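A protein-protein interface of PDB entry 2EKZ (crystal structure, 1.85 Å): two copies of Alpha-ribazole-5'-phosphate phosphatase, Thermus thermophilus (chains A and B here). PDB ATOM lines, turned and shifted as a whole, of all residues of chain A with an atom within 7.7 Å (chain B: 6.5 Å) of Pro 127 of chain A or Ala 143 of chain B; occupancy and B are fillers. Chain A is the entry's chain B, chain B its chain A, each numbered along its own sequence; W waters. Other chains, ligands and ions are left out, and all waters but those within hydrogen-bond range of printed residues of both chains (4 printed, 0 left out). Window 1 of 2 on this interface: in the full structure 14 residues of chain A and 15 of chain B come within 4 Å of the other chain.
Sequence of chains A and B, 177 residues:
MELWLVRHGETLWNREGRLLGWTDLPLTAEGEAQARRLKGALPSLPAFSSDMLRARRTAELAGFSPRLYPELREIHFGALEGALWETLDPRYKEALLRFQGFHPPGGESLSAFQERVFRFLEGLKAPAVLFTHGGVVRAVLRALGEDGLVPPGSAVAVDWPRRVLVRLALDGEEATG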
ATOM      1  N   MET A   1     -12.748  -0.132  -6.759  1.00  0.00           N
ATOM      2  CA  MET A   1     -14.218  -0.066  -6.998  1.00  0.00           C
ATOM      3  C   MET A   1     -14.745  -1.470  -7.263  1.00  0.00           C
ATOM      4  O   MET A   1     -14.253  -2.167  -8.145  1.00  0.00           O
ATOM      5  CB  MET A   1     -14.511   0.848  -8.182  1.00  0.00           C
ATOM      6  CG  MET A   1     -15.982   1.162  -8.354  1.00  0.00           C
ATOM      7  SD  MET A   1     -16.218   2.453  -9.576  1.00  0.00           S
ATOM      8  CE  MET A   1     -16.041   1.497 -11.108  1.00  0.00           C
ATOM      9  N   GLU A   2     -15.756  -1.868  -6.500  1.00  0.00           N
ATOM     10  CA  GLU A   2     -16.321  -3.206  -6.597  1.00  0.00           C
ATOM     11  C   GLU A   2     -17.046  -3.536  -7.891  1.00  0.00           C
ATOM     12  O   GLU A   2     -18.025  -2.887  -8.251  1.00  0.00           O
ATOM     13  CB  GLU A   2     -17.264  -3.456  -5.422  1.00  0.00           C
ATOM     14  CG  GLU A   2     -17.692  -4.907  -5.274  1.00  0.00           C
ATOM     15  CD  GLU A   2     -18.418  -5.157  -3.971  1.00  0.00           C
ATOM     16  OE1 GLU A   2     -17.969  -4.614  -2.943  1.00  0.00           O
ATOM     17  OE2 GLU A   2     -19.423  -5.895  -3.970  1.00  0.00           O
ATOM     18  N   LEU A   3     -16.560  -4.566  -8.574  1.00  0.00           N
ATOM     19  CA  LEU A   3     -17.170  -5.024  -9.812  1.00  0.00           C
ATOM     20  C   LEU A   3     -17.416  -6.518  -9.695  1.00  0.00           C
ATOM     21  O   LEU A   3     -16.546  -7.263  -9.248  1.00  0.00           O
ATOM     22  CB  LEU A   3     -16.249  -4.776 -11.010  1.00  0.00           C
ATOM     23  CG  LEU A   3     -15.885  -3.333 -11.365  1.00  0.00           C
ATOM     24  CD1 LEU A   3     -14.969  -3.341 -12.586  1.00  0.00           C
ATOM     25  CD2 LEU A   3     -17.149  -2.528 -11.640  1.00  0.00           C
ATOM     26  N   TRP A   4     -18.614  -6.951 -10.067  1.00  0.00           N
ATOM     27  CA  TRP A   4     -18.935  -8.367 -10.043  1.00  0.00           C
ATOM     28  C   TRP A   4     -18.955  -8.841 -11.485  1.00  0.00           C
ATOM     29  O   TRP A   4     -19.750  -8.353 -12.286  1.00  0.00           O
ATOM     30  CB  TRP A   4     -20.301  -8.609  -9.397  1.00  0.00           C
ATOM     31  CG  TRP A   4     -20.268  -8.512  -7.912  1.00  0.00           C
ATOM     32  CD1 TRP A   4     -20.175  -7.376  -7.168  1.00  0.00           C
ATOM     33  CD2 TRP A   4     -20.269  -9.603  -6.985  1.00  0.00           C
ATOM     34  NE1 TRP A   4     -20.114  -7.691  -5.828  1.00  0.00           N
ATOM     35  CE2 TRP A   4     -20.171  -9.052  -5.691  1.00  0.00           C
ATOM     36  CE3 TRP A   4     -20.339 -10.995  -7.124  1.00  0.00           C
ATOM     37  CZ2 TRP A   4     -20.142  -9.844  -4.539  1.00  0.00           C
ATOM     38  CZ3 TRP A   4     -20.309 -11.785  -5.974  1.00  0.00           C
ATOM     39  CH2 TRP A   4     -20.210 -11.203  -4.702  1.00  0.00           C
ATOM     40  N   PRO A  43     -25.172  -8.736  -5.361  1.00  0.00           N
ATOM     41  CA  PRO A  43     -25.577  -7.479  -4.727  1.00  0.00           C
ATOM     42  C   PRO A  43     -26.388  -6.645  -5.713  1.00  0.00           C
ATOM     43  O   PRO A  43     -26.195  -6.745  -6.923  1.00  0.00           O
ATOM     44  CB  PRO A  43     -24.245  -6.831  -4.371  1.00  0.00           C
ATOM     45  CG  PRO A  43     -23.355  -7.279  -5.495  1.00  0.00           C
ATOM     46  CD  PRO A  43     -23.723  -8.744  -5.635  1.00  0.00           C
ATOM     47  N   SER A  44     -27.292  -5.826  -5.193  1.00  0.00           N
ATOM     48  CA  SER A  44     -28.133  -4.994  -6.045  1.00  0.00           C
ATOM     49  C   SER A  44     -27.422  -3.730  -6.520  1.00  0.00           C
ATOM     50  O   SER A  44     -27.820  -2.616  -6.185  1.00  0.00           O
ATOM     51  CB  SER A  44     -29.417  -4.629  -5.298  1.00  0.00           C
ATOM     52  OG  SER A  44     -29.119  -4.090  -4.022  1.00  0.00           O
ATOM     53  N   LEU A  45     -26.368  -3.914  -7.311  1.00  0.00           N
ATOM     54  CA  LEU A  45     -25.601  -2.790  -7.849  1.00  0.00           C
ATOM     55  C   LEU A  45     -26.066  -2.508  -9.269  1.00  0.00           C
ATOM     56  O   LEU A  45     -26.776  -3.326  -9.865  1.00  0.00           O
ATOM     57  CB  LEU A  45     -24.110  -3.131  -7.887  1.00  0.00           C
ATOM     58  CG  LEU A  45     -23.497  -3.805  -6.663  1.00  0.00           C
ATOM     59  CD1 LEU A  45     -22.015  -4.038  -6.911  1.00  0.00           C
ATOM     60  CD2 LEU A  45     -23.708  -2.936  -5.427  1.00  0.00           C
ATOM     61  N   PRO A  46     -25.686  -1.342  -9.831  1.00  0.00           N
ATOM     62  CA  PRO A  46     -26.102  -1.037 -11.204  1.00  0.00           C
ATOM     63  C   PRO A  46     -25.642  -2.217 -12.056  1.00  0.00           C
ATOM     64  O   PRO A  46     -24.537  -2.728 -11.865  1.00  0.00           O
ATOM     65  CB  PRO A  46     -25.326   0.234 -11.527  1.00  0.00           C
ATOM     66  CG  PRO A  46     -25.264   0.928 -10.190  1.00  0.00           C
ATOM     67  CD  PRO A  46     -24.926  -0.220  -9.247  1.00  0.00           C
ATOM     68  N   ALA A  47     -26.479  -2.652 -12.988  1.00  0.00           N
ATOM     69  CA  ALA A  47     -26.124  -3.795 -13.819  1.00  0.00           C
ATOM     70  C   ALA A  47     -25.903  -3.460 -15.286  1.00  0.00           C
ATOM     71  O   ALA A  47     -26.560  -2.582 -15.854  1.00  0.00           O
ATOM     72  CB  ALA A  47     -27.197  -4.882 -13.694  1.00  0.00           C
ATOM     73  N   PHE A  48     -24.961  -4.177 -15.888  1.00  0.00           N
ATOM     74  CA  PHE A  48     -24.625  -4.018 -17.296  1.00  0.00           C
ATOM     75  C   PHE A  48     -24.509  -5.431 -17.830  1.00  0.00           C
ATOM     76  O   PHE A  48     -24.188  -6.357 -17.083  1.00  0.00           O
ATOM     77  CB  PHE A  48     -23.287  -3.305 -17.456  1.00  0.00           C
ATOM     78  CG  PHE A  48     -23.281  -1.905 -16.924  1.00  0.00           C
ATOM     79  CD1 PHE A  48     -23.010  -1.662 -15.582  1.00  0.00           C
ATOM     80  CD2 PHE A  48     -23.547  -0.830 -17.761  1.00  0.00           C
ATOM     81  CE1 PHE A  48     -23.002  -0.364 -15.080  1.00  0.00           C
ATOM     82  CE2 PHE A  48     -23.542   0.476 -17.269  1.00  0.00           C
ATOM     83  CZ  PHE A  48     -23.269   0.708 -15.927  1.00  0.00           C
ATOM     84  N   LEU A 124     -16.320   2.748 -16.385  1.00  0.00           N
ATOM     85  CA  LEU A 124     -17.341   2.615 -15.350  1.00  0.00           C
ATOM     86  C   LEU A 124     -17.146   3.697 -14.294  1.00  0.00           C
ATOM     87  O   LEU A 124     -16.024   3.966 -13.872  1.00  0.00           O
ATOM     88  CB  LEU A 124     -17.266   1.222 -14.715  1.00  0.00           C
ATOM     89  CG  LEU A 124     -17.720   0.092 -15.649  1.00  0.00           C
ATOM     90  CD1 LEU A 124     -17.374  -1.273 -15.036  1.00  0.00           C
ATOM     91  CD2 LEU A 124     -19.225   0.213 -15.892  1.00  0.00           C
ATOM     92  N   LYS A 125     -18.248   4.304 -13.865  1.00  0.00           N
ATOM     93  CA  LYS A 125     -18.202   5.385 -12.888  1.00  0.00           C
ATOM     94  C   LYS A 125     -18.768   5.051 -11.513  1.00  0.00           C
ATOM     95  O   LYS A 125     -18.913   5.932 -10.667  1.00  0.00           O
ATOM     96  CB  LYS A 125     -18.926   6.595 -13.469  1.00  0.00           C
ATOM     97  CG  LYS A 125     -18.342   7.021 -14.802  1.00  0.00           C
ATOM     98  CD  LYS A 125     -19.246   7.983 -15.528  1.00  0.00           C
ATOM     99  CE  LYS A 125     -18.716   8.251 -16.926  1.00  0.00           C
ATOM    100  NZ  LYS A 125     -19.655   9.110 -17.683  1.00  0.00           N
ATOM    101  N   ALA A 126     -19.082   3.781 -11.291  1.00  0.00           N
ATOM    102  CA  ALA A 126     -19.613   3.337 -10.007  1.00  0.00           C
ATOM    103  C   ALA A 126     -19.562   1.820  -9.981  1.00  0.00           C
ATOM    104  O   ALA A 126     -19.445   1.186 -11.029  1.00  0.00           O
ATOM    105  CB  ALA A 126     -21.056   3.812  -9.833  1.00  0.00           C
ATOM    106  N   PRO A 127     -19.640   1.217  -8.780  1.00  0.00           N
ATOM    107  CA  PRO A 127     -19.608  -0.244  -8.656  1.00  0.00           C
ATOM    108  C   PRO A 127     -20.692  -0.832  -9.553  1.00  0.00           C
ATOM    109  O   PRO A 127     -21.691  -0.168  -9.834  1.00  0.00           O
ATOM    110  CB  PRO A 127     -19.905  -0.468  -7.178  1.00  0.00           C
ATOM    111  CG  PRO A 127     -19.254   0.739  -6.538  1.00  0.00           C
ATOM    112  CD  PRO A 127     -19.710   1.854  -7.453  1.00  0.00           C
ATOM    113  N   ALA A 128     -20.521  -2.077  -9.982  1.00  0.00           N
ATOM    114  CA  ALA A 128     -21.504  -2.666 -10.871  1.00  0.00           C
ATOM    115  C   ALA A 128     -21.431  -4.180 -10.946  1.00  0.00           C
ATOM    116  O   ALA A 128     -20.447  -4.791 -10.538  1.00  0.00           O
ATOM    117  CB  ALA A 128     -21.316  -2.089 -12.272  1.00  0.00           C
ATOM    118  N   VAL A 129     -22.498  -4.767 -11.472  1.00  0.00           N
ATOM    119  CA  VAL A 129     -22.578  -6.207 -11.692  1.00  0.00           C
ATOM    120  C   VAL A 129     -22.545  -6.313 -13.208  1.00  0.00           C
ATOM    121  O   VAL A 129     -23.361  -5.692 -13.900  1.00  0.00           O
ATOM    122  CB  VAL A 129     -23.895  -6.803 -11.169  1.00  0.00           C
ATOM    123  CG1 VAL A 129     -23.998  -8.285 -11.564  1.00  0.00           C
ATOM    124  CG2 VAL A 129     -23.950  -6.673  -9.661  1.00  0.00           C
ATOM    125  N   LEU A 130     -21.598  -7.093 -13.717  1.00  0.00           N
ATOM    126  CA  LEU A 130     -21.418  -7.251 -15.154  1.00  0.00           C
ATOM    127  C   LEU A 130     -21.735  -8.668 -15.624  1.00  0.00           C
ATOM    128  O   LEU A 130     -21.029  -9.610 -15.279  1.00  0.00           O
ATOM    129  CB  LEU A 130     -19.968  -6.898 -15.515  1.00  0.00           C
ATOM    130  CG  LEU A 130     -19.466  -5.556 -14.956  1.00  0.00           C
ATOM    131  CD1 LEU A 130     -18.001  -5.352 -15.301  1.00  0.00           C
ATOM    132  CD2 LEU A 130     -20.313  -4.424 -15.522  1.00  0.00           C
ATOM    133  N   PHE B 118     -23.704   9.621 -11.300  1.00  0.00           N
ATOM    134  CA  PHE B 118     -22.340   9.129 -11.187  1.00  0.00           C
ATOM    135  C   PHE B 118     -21.347   9.922 -12.025  1.00  0.00           C
ATOM    136  O   PHE B 118     -20.174  10.014 -11.674  1.00  0.00           O
ATOM    137  CB  PHE B 118     -22.292   7.638 -11.536  1.00  0.00           C
ATOM    138  CG  PHE B 118     -23.191   6.793 -10.671  1.00  0.00           C
ATOM    139  CD1 PHE B 118     -23.441   7.152  -9.351  1.00  0.00           C
ATOM    140  CD2 PHE B 118     -23.775   5.637 -11.168  1.00  0.00           C
ATOM    141  CE1 PHE B 118     -24.269   6.370  -8.532  1.00  0.00           C
ATOM    142  CE2 PHE B 118     -24.603   4.846 -10.359  1.00  0.00           C
ATOM    143  CZ  PHE B 118     -24.846   5.218  -9.042  1.00  0.00           C
ATOM    144  N   ARG B 138     -29.976   7.565  -2.529  1.00  0.00           N
ATOM    145  CA  ARG B 138     -30.280   6.148  -2.672  1.00  0.00           C
ATOM    146  C   ARG B 138     -29.420   5.485  -3.738  1.00  0.00           C
ATOM    147  O   ARG B 138     -28.905   4.387  -3.530  1.00  0.00           O
ATOM    148  CB  ARG B 138     -31.758   5.944  -3.007  1.00  0.00           C
ATOM    149  CG  ARG B 138     -32.158   4.483  -2.962  1.00  0.00           C
ATOM    150  CD  ARG B 138     -33.630   4.280  -3.241  1.00  0.00           C
ATOM    151  NE  ARG B 138     -33.965   2.863  -3.157  1.00  0.00           N
ATOM    152  CZ  ARG B 138     -35.063   2.324  -3.673  1.00  0.00           C
ATOM    153  NH1 ARG B 138     -35.940   3.088  -4.312  1.00  0.00           N
ATOM    154  NH2 ARG B 138     -35.271   1.021  -3.564  1.00  0.00           N
ATOM    155  N   ALA B 139     -29.256   6.147  -4.880  1.00  0.00           N
ATOM    156  CA  ALA B 139     -28.444   5.589  -5.961  1.00  0.00           C
ATOM    157  C   ALA B 139     -27.012   5.341  -5.490  1.00  0.00           C
ATOM    158  O   ALA B 139     -26.409   4.317  -5.807  1.00  0.00           O
ATOM    159  CB  ALA B 139     -28.442   6.535  -7.160  1.00  0.00           C
ATOM    160  N   VAL B 140     -26.478   6.294  -4.735  1.00  0.00           N
ATOM    161  CA  VAL B 140     -25.122   6.198  -4.217  1.00  0.00           C
ATOM    162  C   VAL B 140     -25.021   5.085  -3.177  1.00  0.00           C
ATOM    163  O   VAL B 140     -24.111   4.258  -3.227  1.00  0.00           O
ATOM    164  CB  VAL B 140     -24.692   7.550  -3.589  1.00  0.00           C
ATOM    165  CG1 VAL B 140     -23.378   7.396  -2.826  1.00  0.00           C
ATOM    166  CG2 VAL B 140     -24.537   8.588  -4.690  1.00  0.00           C
ATOM    167  N   LEU B 141     -25.962   5.056  -2.240  1.00  0.00           N
ATOM    168  CA  LEU B 141     -25.937   4.025  -1.207  1.00  0.00           C
ATOM    169  C   LEU B 141     -26.063   2.629  -1.800  1.00  0.00           C
ATOM    170  O   LEU B 141     -25.328   1.719  -1.407  1.00  0.00           O
ATOM    171  CB  LEU B 141     -27.057   4.258  -0.191  1.00  0.00           C
ATOM    172  CG  LEU B 141     -26.855   5.472   0.721  1.00  0.00           C
ATOM    173  CD1 LEU B 141     -28.077   5.677   1.591  1.00  0.00           C
ATOM    174  CD2 LEU B 141     -25.618   5.251   1.586  1.00  0.00           C
ATOM    175  N   ARG B 142     -26.994   2.456  -2.737  1.00  0.00           N
ATOM    176  CA  ARG B 142     -27.191   1.153  -3.367  1.00  0.00           C
ATOM    177  C   ARG B 142     -25.979   0.726  -4.188  1.00  0.00           C
ATOM    178  O   ARG B 142     -25.657  -0.462  -4.246  1.00  0.00           O
ATOM    179  CB  ARG B 142     -28.444   1.154  -4.252  1.00  0.00           C
ATOM    180  CG  ARG B 142     -29.749   1.240  -3.474  1.00  0.00           C
ATOM    181  CD  ARG B 142     -30.961   1.095  -4.388  1.00  0.00           C
ATOM    182  NE  ARG B 142     -31.151  -0.272  -4.873  1.00  0.00           N
ATOM    183  CZ  ARG B 142     -31.753  -1.238  -4.182  1.00  0.00           C
ATOM    184  NH1 ARG B 142     -32.231  -0.997  -2.967  1.00  0.00           N
ATOM    185  NH2 ARG B 142     -31.877  -2.448  -4.706  1.00  0.00           N
ATOM    186  N   ALA B 143     -25.304   1.682  -4.823  1.00  0.00           N
ATOM    187  CA  ALA B 143     -24.121   1.356  -5.610  1.00  0.00           C
ATOM    188  C   ALA B 143     -23.029   0.881  -4.661  1.00  0.00           C
ATOM    189  O   ALA B 143     -22.148   0.114  -5.047  1.00  0.00           O
ATOM    190  CB  ALA B 143     -23.641   2.568  -6.392  1.00  0.00           C
ATOM    191  N   LEU B 144     -23.097   1.341  -3.415  1.00  0.00           N
ATOM    192  CA  LEU B 144     -22.118   0.948  -2.405  1.00  0.00           C
ATOM    193  C   LEU B 144     -22.609  -0.253  -1.596  1.00  0.00           C
ATOM    194  O   LEU B 144     -22.088  -0.549  -0.521  1.00  0.00           O
ATOM    195  CB  LEU B 144     -21.802   2.136  -1.482  1.00  0.00           C
ATOM    196  CG  LEU B 144     -21.150   3.328  -2.199  1.00  0.00           C
ATOM    197  CD1 LEU B 144     -20.964   4.494  -1.236  1.00  0.00           C
ATOM    198  CD2 LEU B 144     -19.808   2.911  -2.779  1.00  0.00           C
ATOM    199  N   GLY B 145     -23.625  -0.929  -2.125  1.00  0.00           N
ATOM    200  CA  GLY B 145     -24.164  -2.120  -1.491  1.00  0.00           C
ATOM    201  C   GLY B 145     -24.957  -1.993  -0.204  1.00  0.00           C
ATOM    202  O   GLY B 145     -25.005  -2.949   0.572  1.00  0.00           O
ATOM    203  N   GLU B 146     -25.589  -0.846   0.030  1.00  0.00           N
ATOM    204  CA  GLU B 146     -26.374  -0.660   1.251  1.00  0.00           C
ATOM    205  C   GLU B 146     -27.779  -0.143   0.970  1.00  0.00           C
ATOM    206  O   GLU B 146     -28.055   0.368  -0.110  1.00  0.00           O
ATOM    207  CB  GLU B 146     -25.672   0.320   2.192  1.00  0.00           C
ATOM    208  CG  GLU B 146     -24.221  -0.010   2.484  1.00  0.00           C
ATOM    209  CD  GLU B 146     -23.670   0.796   3.645  1.00  0.00           C
ATOM    210  OE1 GLU B 146     -24.336   1.761   4.070  1.00  0.00           O
ATOM    211  OE2 GLU B 146     -22.570   0.467   4.131  1.00  0.00           O
ATOM    212  N   TRP B 160     -16.273   7.865  -1.896  1.00  0.00           N
ATOM    213  CA  TRP B 160     -16.669   7.481  -3.252  1.00  0.00           C
ATOM    214  C   TRP B 160     -15.487   7.080  -4.126  1.00  0.00           C
ATOM    215  O   TRP B 160     -14.484   7.787  -4.175  1.00  0.00           O
ATOM    216  CB  TRP B 160     -17.425   8.643  -3.907  1.00  0.00           C
ATOM    217  CG  TRP B 160     -18.013   8.298  -5.232  1.00  0.00           C
ATOM    218  CD1 TRP B 160     -17.589   8.727  -6.459  1.00  0.00           C
ATOM    219  CD2 TRP B 160     -19.115   7.417  -5.470  1.00  0.00           C
ATOM    220  NE1 TRP B 160     -18.362   8.161  -7.450  1.00  0.00           N
ATOM    221  CE2 TRP B 160     -19.305   7.352  -6.871  1.00  0.00           C
ATOM    222  CE3 TRP B 160     -19.961   6.672  -4.636  1.00  0.00           C
ATOM    223  CZ2 TRP B 160     -20.305   6.570  -7.456  1.00  0.00           C
ATOM    224  CZ3 TRP B 160     -20.957   5.892  -5.220  1.00  0.00           C
ATOM    225  CH2 TRP B 160     -21.119   5.849  -6.619  1.00  0.00           C
ATOM    226  N   PRO B 161     -15.608   5.966  -4.871  1.00  0.00           N
ATOM    227  CA  PRO B 161     -16.726   5.025  -5.004  1.00  0.00           C
ATOM    228  C   PRO B 161     -16.458   3.717  -4.265  1.00  0.00           C
ATOM    229  O   PRO B 161     -16.701   2.634  -4.804  1.00  0.00           O
ATOM    230  CB  PRO B 161     -16.768   4.798  -6.505  1.00  0.00           C
ATOM    231  CG  PRO B 161     -15.277   4.633  -6.792  1.00  0.00           C
ATOM    232  CD  PRO B 161     -14.609   5.720  -5.928  1.00  0.00           C
ATOM    233  N   ARG B 162     -15.982   3.814  -3.029  1.00  0.00           N
ATOM    234  CA  ARG B 162     -15.631   2.620  -2.274  1.00  0.00           C
ATOM    235  C   ARG B 162     -16.533   2.181  -1.132  1.00  0.00           C
ATOM    236  O   ARG B 162     -16.881   1.000  -1.053  1.00  0.00           O
ATOM    237  CB  ARG B 162     -14.195   2.756  -1.750  1.00  0.00           C
ATOM    238  CG  ARG B 162     -13.160   2.921  -2.853  1.00  0.00           C
ATOM    239  CD  ARG B 162     -11.748   3.077  -2.297  1.00  0.00           C
ATOM    240  NE  ARG B 162     -11.238   1.835  -1.718  1.00  0.00           N
ATOM    241  CZ  ARG B 162     -10.932   0.745  -2.420  1.00  0.00           C
ATOM    242  NH1 ARG B 162     -11.081   0.733  -3.738  1.00  0.00           N
ATOM    243  NH2 ARG B 162     -10.472  -0.337  -1.802  1.00  0.00           N
HETATM  244  O   HOH W   1     -27.099  -2.448  -3.121  1.00  0.00           O
HETATM  245  O   HOH W   2     -18.332   8.437 -10.268  1.00  0.00           O
HETATM  246  O   HOH W   3     -11.702   2.407  -6.041  1.00  0.00           O
HETATM  247  O   HOH W   4     -16.923  -0.262  -4.410  1.00  0.00           O
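Among the printed residues, pairs that only touch across the chains: Pro 127 of chain A with Ala 143 of chain B (3.1 Å), Leu 45 of chain A with Arg 142 of chain B (3.4 Å), Leu 45 of chain A with Ala 143 of chain B (3.4 Å), Ala 126 of chain A with Phe 118 of chain B (3.5 Å), Met 1 of chain A with Arg 162 of chain B (3.6 Å), Lys 125 of chain A with Trp 160 of chain B (3.6 Å), Pro 127 of chain A with Pro 161 of chain B (3.6 Å), Met 1 of chain A with Pro 161 of chain B (3.7 Å), Ala 126 of chain A with Trp 160 of chain B (3.7 Å), Leu 45 of chain A with Gly 145 of chain B (3.9 Å), Lys 125 of chain A with Phe 118 of chain B (3.9 Å) and Pro 46 of chain A with Phe 118 of chain B (3.98 Å).
Pro 127 of chain A touches just these residues of chain B: Ala 143 and Pro 161.
Ala 143 of chain B touches two residues of chain A.
Printed residues of chain A within 4 Å of Arg 142 of chain B: Ser 44 and Leu 45.
Of the printed residues of chain A, Arg 162 of chain B touches Met 1 (3.6 Å).
Printed residues of chain B within 4 Å of Ser 44 of chain A: Arg 142.
The guanidinium group of Arg 142 of chain B is in hydrogen-bond range of the side-chain hydroxyl of Ser 44 of chain A.
The backbone NH of Ala 126 of chain A lies close to the side-chain sulfur of Met 1 of chain A.
The backbone carbonyl oxygen (O) of Pro 46 of chain A is in hydrogen-bond range of the backbone NH (N) of Val 129 of chain A (2.9 Å).
No position is printed for both chains.
Water W2 lies within hydrogen-bond range of O of Lys 125 of chain A (2.6 Å), O of Phe 118 of chain B (2.8 Å) and NE1 of Trp 160 of chain B (2.8 Å).
Water W1 bridges the backbone carbonyl oxygen (O) of Arg 142 of chain B (2.7 Å) and the side-chain hydroxyl (OG) of Ser 44 of chain A (2.8 Å).
Water W3 bridges N of Met 1 of chain A and NH1 of Arg 162 of chain B.
Water W4 lies within hydrogen-bond range of N of Glu 2 of chain A and O of Pro 161 of chain B.
Printed residues of chain B that touch a printed residue of chain A: Phe 118, Arg 142, Ala 143, Gly 145, Trp 160, Pro 161 and Arg 162.
Along chain B the printed residues that touch a printed residue of chain A span positions 118 to 162.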
